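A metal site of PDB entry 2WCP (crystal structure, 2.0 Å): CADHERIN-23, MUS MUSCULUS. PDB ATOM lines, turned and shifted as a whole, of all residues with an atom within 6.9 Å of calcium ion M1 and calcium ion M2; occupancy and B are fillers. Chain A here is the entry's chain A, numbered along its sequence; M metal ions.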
ATOM      1  N   GLU A  22      -6.567  14.775 -26.509  1.00  0.00           N
ATOM      2  CA  GLU A  22      -7.300  15.512 -25.495  1.00  0.00           C
ATOM      3  C   GLU A  22      -6.707  16.884 -25.216  1.00  0.00           C
ATOM      4  O   GLU A  22      -7.400  17.701 -24.646  1.00  0.00           O
ATOM      5  CB  GLU A  22      -7.468  14.723 -24.209  1.00  0.00           C
ATOM      6  CG  GLU A  22      -6.173  14.490 -23.416  1.00  0.00           C
ATOM      7  CD  GLU A  22      -6.394  13.749 -22.125  1.00  0.00           C
ATOM      8  OE1 GLU A  22      -5.508  12.941 -21.720  1.00  0.00           O
ATOM      9  OE2 GLU A  22      -7.439  13.995 -21.481  1.00  0.00           O
ATOM     10  N   ASP A  72     -11.561  15.385 -22.704  1.00  0.00           N
ATOM     11  CA  ASP A  72     -10.894  14.885 -21.490  1.00  0.00           C
ATOM     12  C   ASP A  72     -11.016  13.372 -21.539  1.00  0.00           C
ATOM     13  O   ASP A  72     -12.066  12.830 -21.240  1.00  0.00           O
ATOM     14  CB  ASP A  72     -11.555  15.452 -20.233  1.00  0.00           C
ATOM     15  CG  ASP A  72     -10.971  14.864 -18.926  1.00  0.00           C
ATOM     16  OD1 ASP A  72     -11.580  15.037 -17.873  1.00  0.00           O
ATOM     17  OD2 ASP A  72      -9.914  14.199 -18.981  1.00  0.00           O
ATOM     18  N   ARG A  73      -9.943  12.680 -21.949  1.00  0.00           N
ATOM     19  CA  ARG A  73      -9.995  11.251 -22.131  1.00  0.00           C
ATOM     20  C   ARG A  73     -10.405  10.532 -20.854  1.00  0.00           C
ATOM     21  O   ARG A  73     -11.020   9.488 -20.917  1.00  0.00           O
ATOM     22  CB  ARG A  73      -8.640  10.693 -22.611  1.00  0.00           C
ATOM     23  CG  ARG A  73      -8.687   9.225 -23.109  1.00  0.00           C
ATOM     24  CD  ARG A  73      -7.288   8.602 -23.134  1.00  0.00           C
ATOM     25  NE  ARG A  73      -6.827   8.496 -21.764  1.00  0.00           N
ATOM     26  CZ  ARG A  73      -7.151   7.515 -20.939  1.00  0.00           C
ATOM     27  NH1 ARG A  73      -6.770   7.565 -19.671  1.00  0.00           N
ATOM     28  NH2 ARG A  73      -7.894   6.499 -21.359  1.00  0.00           N
ATOM     29  N   GLU A  74     -10.056  11.098 -19.692  1.00  0.00           N
ATOM     30  CA  GLU A  74     -10.366  10.494 -18.405  1.00  0.00           C
ATOM     31  C   GLU A  74     -11.834  10.682 -18.013  1.00  0.00           C
ATOM     32  O   GLU A  74     -12.292  10.050 -17.098  1.00  0.00           O
ATOM     33  CB  GLU A  74      -9.436  11.031 -17.294  1.00  0.00           C
ATOM     34  CG  GLU A  74      -7.988  10.464 -17.344  1.00  0.00           C
ATOM     35  CD  GLU A  74      -7.096  11.053 -18.420  1.00  0.00           C
ATOM     36  OE1 GLU A  74      -6.324  10.302 -19.064  1.00  0.00           O
ATOM     37  OE2 GLU A  74      -7.101  12.269 -18.642  1.00  0.00           O
ATOM     38  N   GLY A 101      -7.250  10.853 -27.682  1.00  0.00           N
ATOM     39  CA  GLY A 101      -5.861  10.483 -27.378  1.00  0.00           C
ATOM     40  C   GLY A 101      -5.410  11.024 -26.039  1.00  0.00           C
ATOM     41  O   GLY A 101      -5.778  12.131 -25.635  1.00  0.00           O
ATOM     42  N   ASP A 102      -4.616  10.209 -25.333  1.00  0.00           N
ATOM     43  CA  ASP A 102      -4.172  10.581 -24.022  1.00  0.00           C
ATOM     44  C   ASP A 102      -3.016  11.544 -24.025  1.00  0.00           C
ATOM     45  O   ASP A 102      -2.112  11.463 -24.861  1.00  0.00           O
ATOM     46  CB  ASP A 102      -3.751   9.332 -23.255  1.00  0.00           C
ATOM     47  CG  ASP A 102      -3.552   9.596 -21.802  1.00  0.00           C
ATOM     48  OD1 ASP A 102      -4.477  10.145 -21.127  1.00  0.00           O
ATOM     49  OD2 ASP A 102      -2.467   9.256 -21.310  1.00  0.00           O
ATOM     50  N   VAL A 103      -3.051  12.468 -23.071  1.00  0.00           N
ATOM     51  CA  VAL A 103      -1.874  13.235 -22.694  1.00  0.00           C
ATOM     52  C   VAL A 103      -1.708  13.030 -21.179  1.00  0.00           C
ATOM     53  O   VAL A 103      -2.673  12.684 -20.459  1.00  0.00           O
ATOM     54  CB  VAL A 103      -2.026  14.711 -23.128  1.00  0.00           C
ATOM     55  CG1 VAL A 103      -1.252  15.642 -22.234  1.00  0.00           C
ATOM     56  CG2 VAL A 103      -1.606  14.899 -24.612  1.00  0.00           C
ATOM     57  N   ASN A 104      -0.479  13.205 -20.684  1.00  0.00           N
ATOM     58  CA  ASN A 104      -0.260  13.102 -19.260  1.00  0.00           C
ATOM     59  C   ASN A 104      -0.727  14.358 -18.556  1.00  0.00           C
ATOM     60  O   ASN A 104       0.065  15.280 -18.378  1.00  0.00           O
ATOM     61  CB  ASN A 104       1.213  12.868 -18.923  1.00  0.00           C
ATOM     62  CG  ASN A 104       1.408  12.600 -17.445  1.00  0.00           C
ATOM     63  OD1 ASN A 104       0.533  11.958 -16.858  1.00  0.00           O
ATOM     64  ND2 ASN A 104       2.514  13.069 -16.837  1.00  0.00           N
ATOM     65  N   ASP A 105      -1.993  14.411 -18.161  1.00  0.00           N
ATOM     66  CA  ASP A 105      -2.560  15.635 -17.591  1.00  0.00           C
ATOM     67  C   ASP A 105      -3.105  15.433 -16.167  1.00  0.00           C
ATOM     68  O   ASP A 105      -3.778  16.323 -15.640  1.00  0.00           O
ATOM     69  CB  ASP A 105      -3.600  16.282 -18.553  1.00  0.00           C
ATOM     70  CG  ASP A 105      -4.744  15.348 -18.939  1.00  0.00           C
ATOM     71  OD1 ASP A 105      -4.685  14.095 -18.742  1.00  0.00           O
ATOM     72  OD2 ASP A 105      -5.747  15.894 -19.481  1.00  0.00           O
ATOM     73  N   ASN A 106      -2.801  14.299 -15.537  1.00  0.00           N
ATOM     74  CA  ASN A 106      -3.204  14.048 -14.161  1.00  0.00           C
ATOM     75  C   ASN A 106      -2.004  13.719 -13.277  1.00  0.00           C
ATOM     76  O   ASN A 106      -1.135  12.959 -13.691  1.00  0.00           O
ATOM     77  CB  ASN A 106      -4.179  12.887 -14.110  1.00  0.00           C
ATOM     78  CG  ASN A 106      -5.470  13.181 -14.806  1.00  0.00           C
ATOM     79  OD1 ASN A 106      -5.602  12.975 -16.043  1.00  0.00           O
ATOM     80  ND2 ASN A 106      -6.438  13.636 -14.050  1.00  0.00           N
ATOM     81  N   ALA A 107      -1.967  14.291 -12.080  1.00  0.00           N
ATOM     82  CA  ALA A 107      -1.035  13.835 -11.025  1.00  0.00           C
ATOM     83  C   ALA A 107      -1.665  12.670 -10.295  1.00  0.00           C
ATOM     84  O   ALA A 107      -2.881  12.487 -10.349  1.00  0.00           O
ATOM     85  CB  ALA A 107      -0.722  14.962 -10.013  1.00  0.00           C
ATOM     86  N   PRO A 108      -0.850  11.862  -9.588  1.00  0.00           N
ATOM     87  CA  PRO A 108      -1.438  10.771  -8.852  1.00  0.00           C
ATOM     88  C   PRO A 108      -2.313  11.283  -7.709  1.00  0.00           C
ATOM     89  O   PRO A 108      -2.112  12.392  -7.231  1.00  0.00           O
ATOM     90  CB  PRO A 108      -0.214  10.016  -8.305  1.00  0.00           C
ATOM     91  CG  PRO A 108       0.901  10.390  -9.246  1.00  0.00           C
ATOM     92  CD  PRO A 108       0.628  11.798  -9.615  1.00  0.00           C
ATOM     93  N   ASP A 136      -3.196   6.806 -10.860  1.00  0.00           N
ATOM     94  CA  ASP A 136      -2.971   7.843 -11.879  1.00  0.00           C
ATOM     95  C   ASP A 136      -3.686   7.346 -13.119  1.00  0.00           C
ATOM     96  O   ASP A 136      -3.356   6.276 -13.630  1.00  0.00           O
ATOM     97  CB  ASP A 136      -1.464   8.059 -12.097  1.00  0.00           C
ATOM     98  CG  ASP A 136      -1.165   9.271 -12.958  1.00  0.00           C
ATOM     99  OD1 ASP A 136      -1.883   9.472 -13.953  1.00  0.00           O
ATOM    100  OD2 ASP A 136      -0.219  10.006 -12.691  1.00  0.00           O
ATOM    101  N   PRO A 137      -4.740   8.062 -13.551  1.00  0.00           N
ATOM    102  CA  PRO A 137      -5.596   7.538 -14.611  1.00  0.00           C
ATOM    103  C   PRO A 137      -5.029   7.747 -16.035  1.00  0.00           C
ATOM    104  O   PRO A 137      -5.627   7.295 -17.010  1.00  0.00           O
ATOM    105  CB  PRO A 137      -6.882   8.326 -14.399  1.00  0.00           C
ATOM    106  CG  PRO A 137      -6.393   9.645 -13.933  1.00  0.00           C
ATOM    107  CD  PRO A 137      -5.195   9.369 -13.064  1.00  0.00           C
ATOM    108  N   ASP A 138      -3.898   8.383 -16.184  1.00  0.00           N
ATOM    109  CA  ASP A 138      -3.316   8.541 -17.532  1.00  0.00           C
ATOM    110  C   ASP A 138      -2.773   7.226 -18.072  1.00  0.00           C
ATOM    111  O   ASP A 138      -2.715   6.245 -17.353  1.00  0.00           O
ATOM    112  CB  ASP A 138      -2.236   9.598 -17.535  1.00  0.00           C
ATOM    113  CG  ASP A 138      -2.756  10.954 -17.132  1.00  0.00           C
ATOM    114  OD1 ASP A 138      -3.728  11.463 -17.758  1.00  0.00           O
ATOM    115  OD2 ASP A 138      -2.171  11.526 -16.204  1.00  0.00           O
ATOM    116  N   LEU A 139      -2.421   7.201 -19.357  1.00  0.00           N
ATOM    117  CA  LEU A 139      -2.003   5.946 -19.990  1.00  0.00           C
ATOM    118  C   LEU A 139      -0.480   5.839 -19.981  1.00  0.00           C
ATOM    119  O   LEU A 139       0.228   6.819 -19.836  1.00  0.00           O
ATOM    120  CB  LEU A 139      -2.542   5.825 -21.403  1.00  0.00           C
ATOM    121  CG  LEU A 139      -4.079   5.803 -21.525  1.00  0.00           C
ATOM    122  CD1 LEU A 139      -4.487   5.491 -22.971  1.00  0.00           C
ATOM    123  CD2 LEU A 139      -4.736   4.798 -20.537  1.00  0.00           C
ATOM    124  N   ALA A 141       3.418   5.380 -19.329  1.00  0.00           N
ATOM    125  CA  ALA A 141       4.343   5.834 -18.288  1.00  0.00           C
ATOM    126  C   ALA A 141       3.726   6.946 -17.446  1.00  0.00           C
ATOM    127  O   ALA A 141       3.958   7.027 -16.244  1.00  0.00           O
ATOM    128  CB  ALA A 141       5.648   6.317 -18.908  1.00  0.00           C
ATOM    129  N   GLY A 142       2.911   7.797 -18.079  1.00  0.00           N
ATOM    130  CA  GLY A 142       2.212   8.864 -17.352  1.00  0.00           C
ATOM    131  C   GLY A 142       1.172   8.379 -16.354  1.00  0.00           C
ATOM    132  O   GLY A 142       0.664   9.160 -15.529  1.00  0.00           O
ATOM    133  N   GLY A 143       0.825   7.110 -16.434  1.00  0.00           N
ATOM    134  CA  GLY A 143      -0.105   6.502 -15.501  1.00  0.00           C
ATOM    135  C   GLY A 143       0.537   5.511 -14.529  1.00  0.00           C
ATOM    136  O   GLY A 143      -0.178   4.827 -13.787  1.00  0.00           O
ATOM    137  N   SER A 144       1.871   5.426 -14.526  1.00  0.00           N
ATOM    138  CA  SER A 144       2.590   4.394 -13.761  1.00  0.00           C
ATOM    139  C   SER A 144       3.310   5.063 -12.613  1.00  0.00           C
ATOM    140  O   SER A 144       4.227   5.833 -12.835  1.00  0.00           O
ATOM    141  CB  SER A 144       3.571   3.669 -14.686  1.00  0.00           C
ATOM    142  OG  SER A 144       4.424   2.841 -13.941  1.00  0.00           O
ATOM    143  N   ASP A 187       4.246  10.066 -11.458  1.00  0.00           N
ATOM    144  CA  ASP A 187       4.117   9.231 -12.622  1.00  0.00           C
ATOM    145  C   ASP A 187       5.477   9.242 -13.293  1.00  0.00           C
ATOM    146  O   ASP A 187       6.332  10.021 -12.920  1.00  0.00           O
ATOM    147  CB  ASP A 187       2.961   9.662 -13.586  1.00  0.00           C
ATOM    148  CG  ASP A 187       3.099  11.069 -14.102  1.00  0.00           C
ATOM    149  OD1 ASP A 187       4.220  11.437 -14.500  1.00  0.00           O
ATOM    150  OD2 ASP A 187       2.082  11.807 -14.120  1.00  0.00           O
ATOM    151  N   GLN A 188       5.664   8.388 -14.282  1.00  0.00           N
ATOM    152  CA  GLN A 188       6.924   8.285 -14.964  1.00  0.00           C
ATOM    153  C   GLN A 188       6.923   8.869 -16.370  1.00  0.00           C
ATOM    154  O   GLN A 188       7.605   8.362 -17.258  1.00  0.00           O
ATOM    155  CB  GLN A 188       7.317   6.819 -15.005  1.00  0.00           C
ATOM    156  CG  GLN A 188       7.645   6.263 -13.610  1.00  0.00           C
ATOM    157  CD  GLN A 188       7.844   4.793 -13.689  1.00  0.00           C
ATOM    158  OE1 GLN A 188       6.950   4.018 -13.357  1.00  0.00           O
ATOM    159  NE2 GLN A 188       8.988   4.387 -14.221  1.00  0.00           N
ATOM    160  N   ASP A 189       6.156   9.944 -16.587  1.00  0.00           N
ATOM    161  CA  ASP A 189       6.190  10.596 -17.905  1.00  0.00           C
ATOM    162  C   ASP A 189       7.584  11.186 -18.123  1.00  0.00           C
ATOM    163  O   ASP A 189       8.112  11.920 -17.298  1.00  0.00           O
ATOM    164  CB  ASP A 189       5.144  11.686 -18.036  1.00  0.00           C
ATOM    165  CG  ASP A 189       4.975  12.169 -19.471  1.00  0.00           C
ATOM    166  OD1 ASP A 189       4.404  11.424 -20.317  1.00  0.00           O
ATOM    167  OD2 ASP A 189       5.392  13.312 -19.747  1.00  0.00           O
ATOM    168  N   ARG A 192       7.252  15.191 -19.089  1.00  0.00           N
ATOM    169  CA  ARG A 192       6.628  16.029 -18.046  1.00  0.00           C
ATOM    170  C   ARG A 192       5.972  15.253 -16.903  1.00  0.00           C
ATOM    171  O   ARG A 192       4.747  15.179 -16.824  1.00  0.00           O
ATOM    172  CB  ARG A 192       5.618  16.993 -18.674  1.00  0.00           C
ATOM    173  CG  ARG A 192       5.135  18.104 -17.734  1.00  0.00           C
ATOM    174  CD  ARG A 192       4.397  19.213 -18.521  1.00  0.00           C
ATOM    175  NE  ARG A 192       3.509  20.022 -17.668  1.00  0.00           N
ATOM    176  CZ  ARG A 192       2.313  19.619 -17.212  1.00  0.00           C
ATOM    177  NH1 ARG A 192       1.597  20.441 -16.451  1.00  0.00           N
ATOM    178  NH2 ARG A 192       1.848  18.410 -17.486  1.00  0.00           N
ATOM    179  N   PRO A 193       6.781  14.690 -15.998  1.00  0.00           N
ATOM    180  CA  PRO A 193       6.196  13.927 -14.895  1.00  0.00           C
ATOM    181  C   PRO A 193       5.361  14.801 -13.966  1.00  0.00           C
ATOM    182  O   PRO A 193       5.665  15.964 -13.775  1.00  0.00           O
ATOM    183  CB  PRO A 193       7.406  13.367 -14.157  1.00  0.00           C
ATOM    184  CG  PRO A 193       8.547  14.239 -14.532  1.00  0.00           C
ATOM    185  CD  PRO A 193       8.238  14.847 -15.871  1.00  0.00           C
ATOM    186  N   LEU A 194       4.305  14.230 -13.389  1.00  0.00           N
ATOM    187  CA  LEU A 194       3.483  14.927 -12.438  1.00  0.00           C
ATOM    188  C   LEU A 194       3.513  14.104 -11.138  1.00  0.00           C
ATOM    189  O   LEU A 194       3.579  12.877 -11.190  1.00  0.00           O
ATOM    190  CB  LEU A 194       2.057  15.040 -12.950  1.00  0.00           C
ATOM    191  CG  LEU A 194       1.943  15.790 -14.296  1.00  0.00           C
ATOM    192  CD1 LEU A 194       0.504  15.805 -14.728  1.00  0.00           C
ATOM    193  CD2 LEU A 194       2.476  17.194 -14.134  1.00  0.00           C
HETATM  194 CA    CA M   1      -0.274  11.079 -14.789  1.00  0.00          CA
HETATM  195 CA    CA M   2      -4.832  11.973 -19.741  1.00  0.00          CA
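Calcium ion M1 is bound by the backbone carbonyl oxygen (O) of Gly 142 (2.3 Å), the backbone carbonyl oxygen (O) of Asn 106 (2.3 Å), the side-chain carboxylate (OD2) of Asp 136 (2.4 Å), the side-chain amide oxygen (OD1) of Asn 104 (2.4 Å), the side-chain carboxylate (OD2) of Asp 138 (2.4 Å), the side-chain carboxylate (OD1) of Asp 136 (2.4 Å) and the side-chain carboxylate (OD2) of Asp 187 (2.6 Å).
OE1 of Glu 74 lies close to NH1 of Arg 73 (2.8 Å). The side-chain amide oxygen (OD1) of Asn 106 lies close to the side-chain carboxylate (OD1) of Asp 105, at 3.1 Å. The backbone NH of Asp 187 is in hydrogen-bond range of the backbone carbonyl oxygen of Leu 194 (2.9 Å). The backbone NH (N) of Glu 22 lies within hydrogen-bond range of the backbone carbonyl oxygen (O) of Gly 101, 2.9 Å away. The guanidinium group of Arg 73 lies close to the side-chain carboxylate of Asp 102 (2.9 Å). The side-chain carboxylate (OE2) of Glu 22 sits at hydrogen-bond distance from the backbone NH (N) of Arg 73 (2.9 Å). The side-chain carboxylate of Asp 102 sits at hydrogen-bond distance from the backbone NH of Leu 139. OE2 of Glu 74 lies close to OD1 of Asn 106, at 3.1 Å.
The nearest printed residue that does not touch calcium ion M1 is Gly 143 (4.4 Å).
Calcium ion M2 is bound by OE1 of Glu 22 (2.3 Å), OD1 of Asp 102 (2.3 Å), OD1 of Asp 138 (2.3 Å), OE1 of Glu 74 (2.3 Å), OD1 of Asp 105 (2.3 Å), O of Val 103 (2.4 Å) and OE2 of Glu 74 (2.5 Å). Calcium ion M2 has seven donor atoms within binding distance.
Of the 26 residues printed, 7 come within 4 Å of calcium ion M2. The nearest printed residue that does not touch calcium ion M2 is Arg 73 (4.5 Å).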
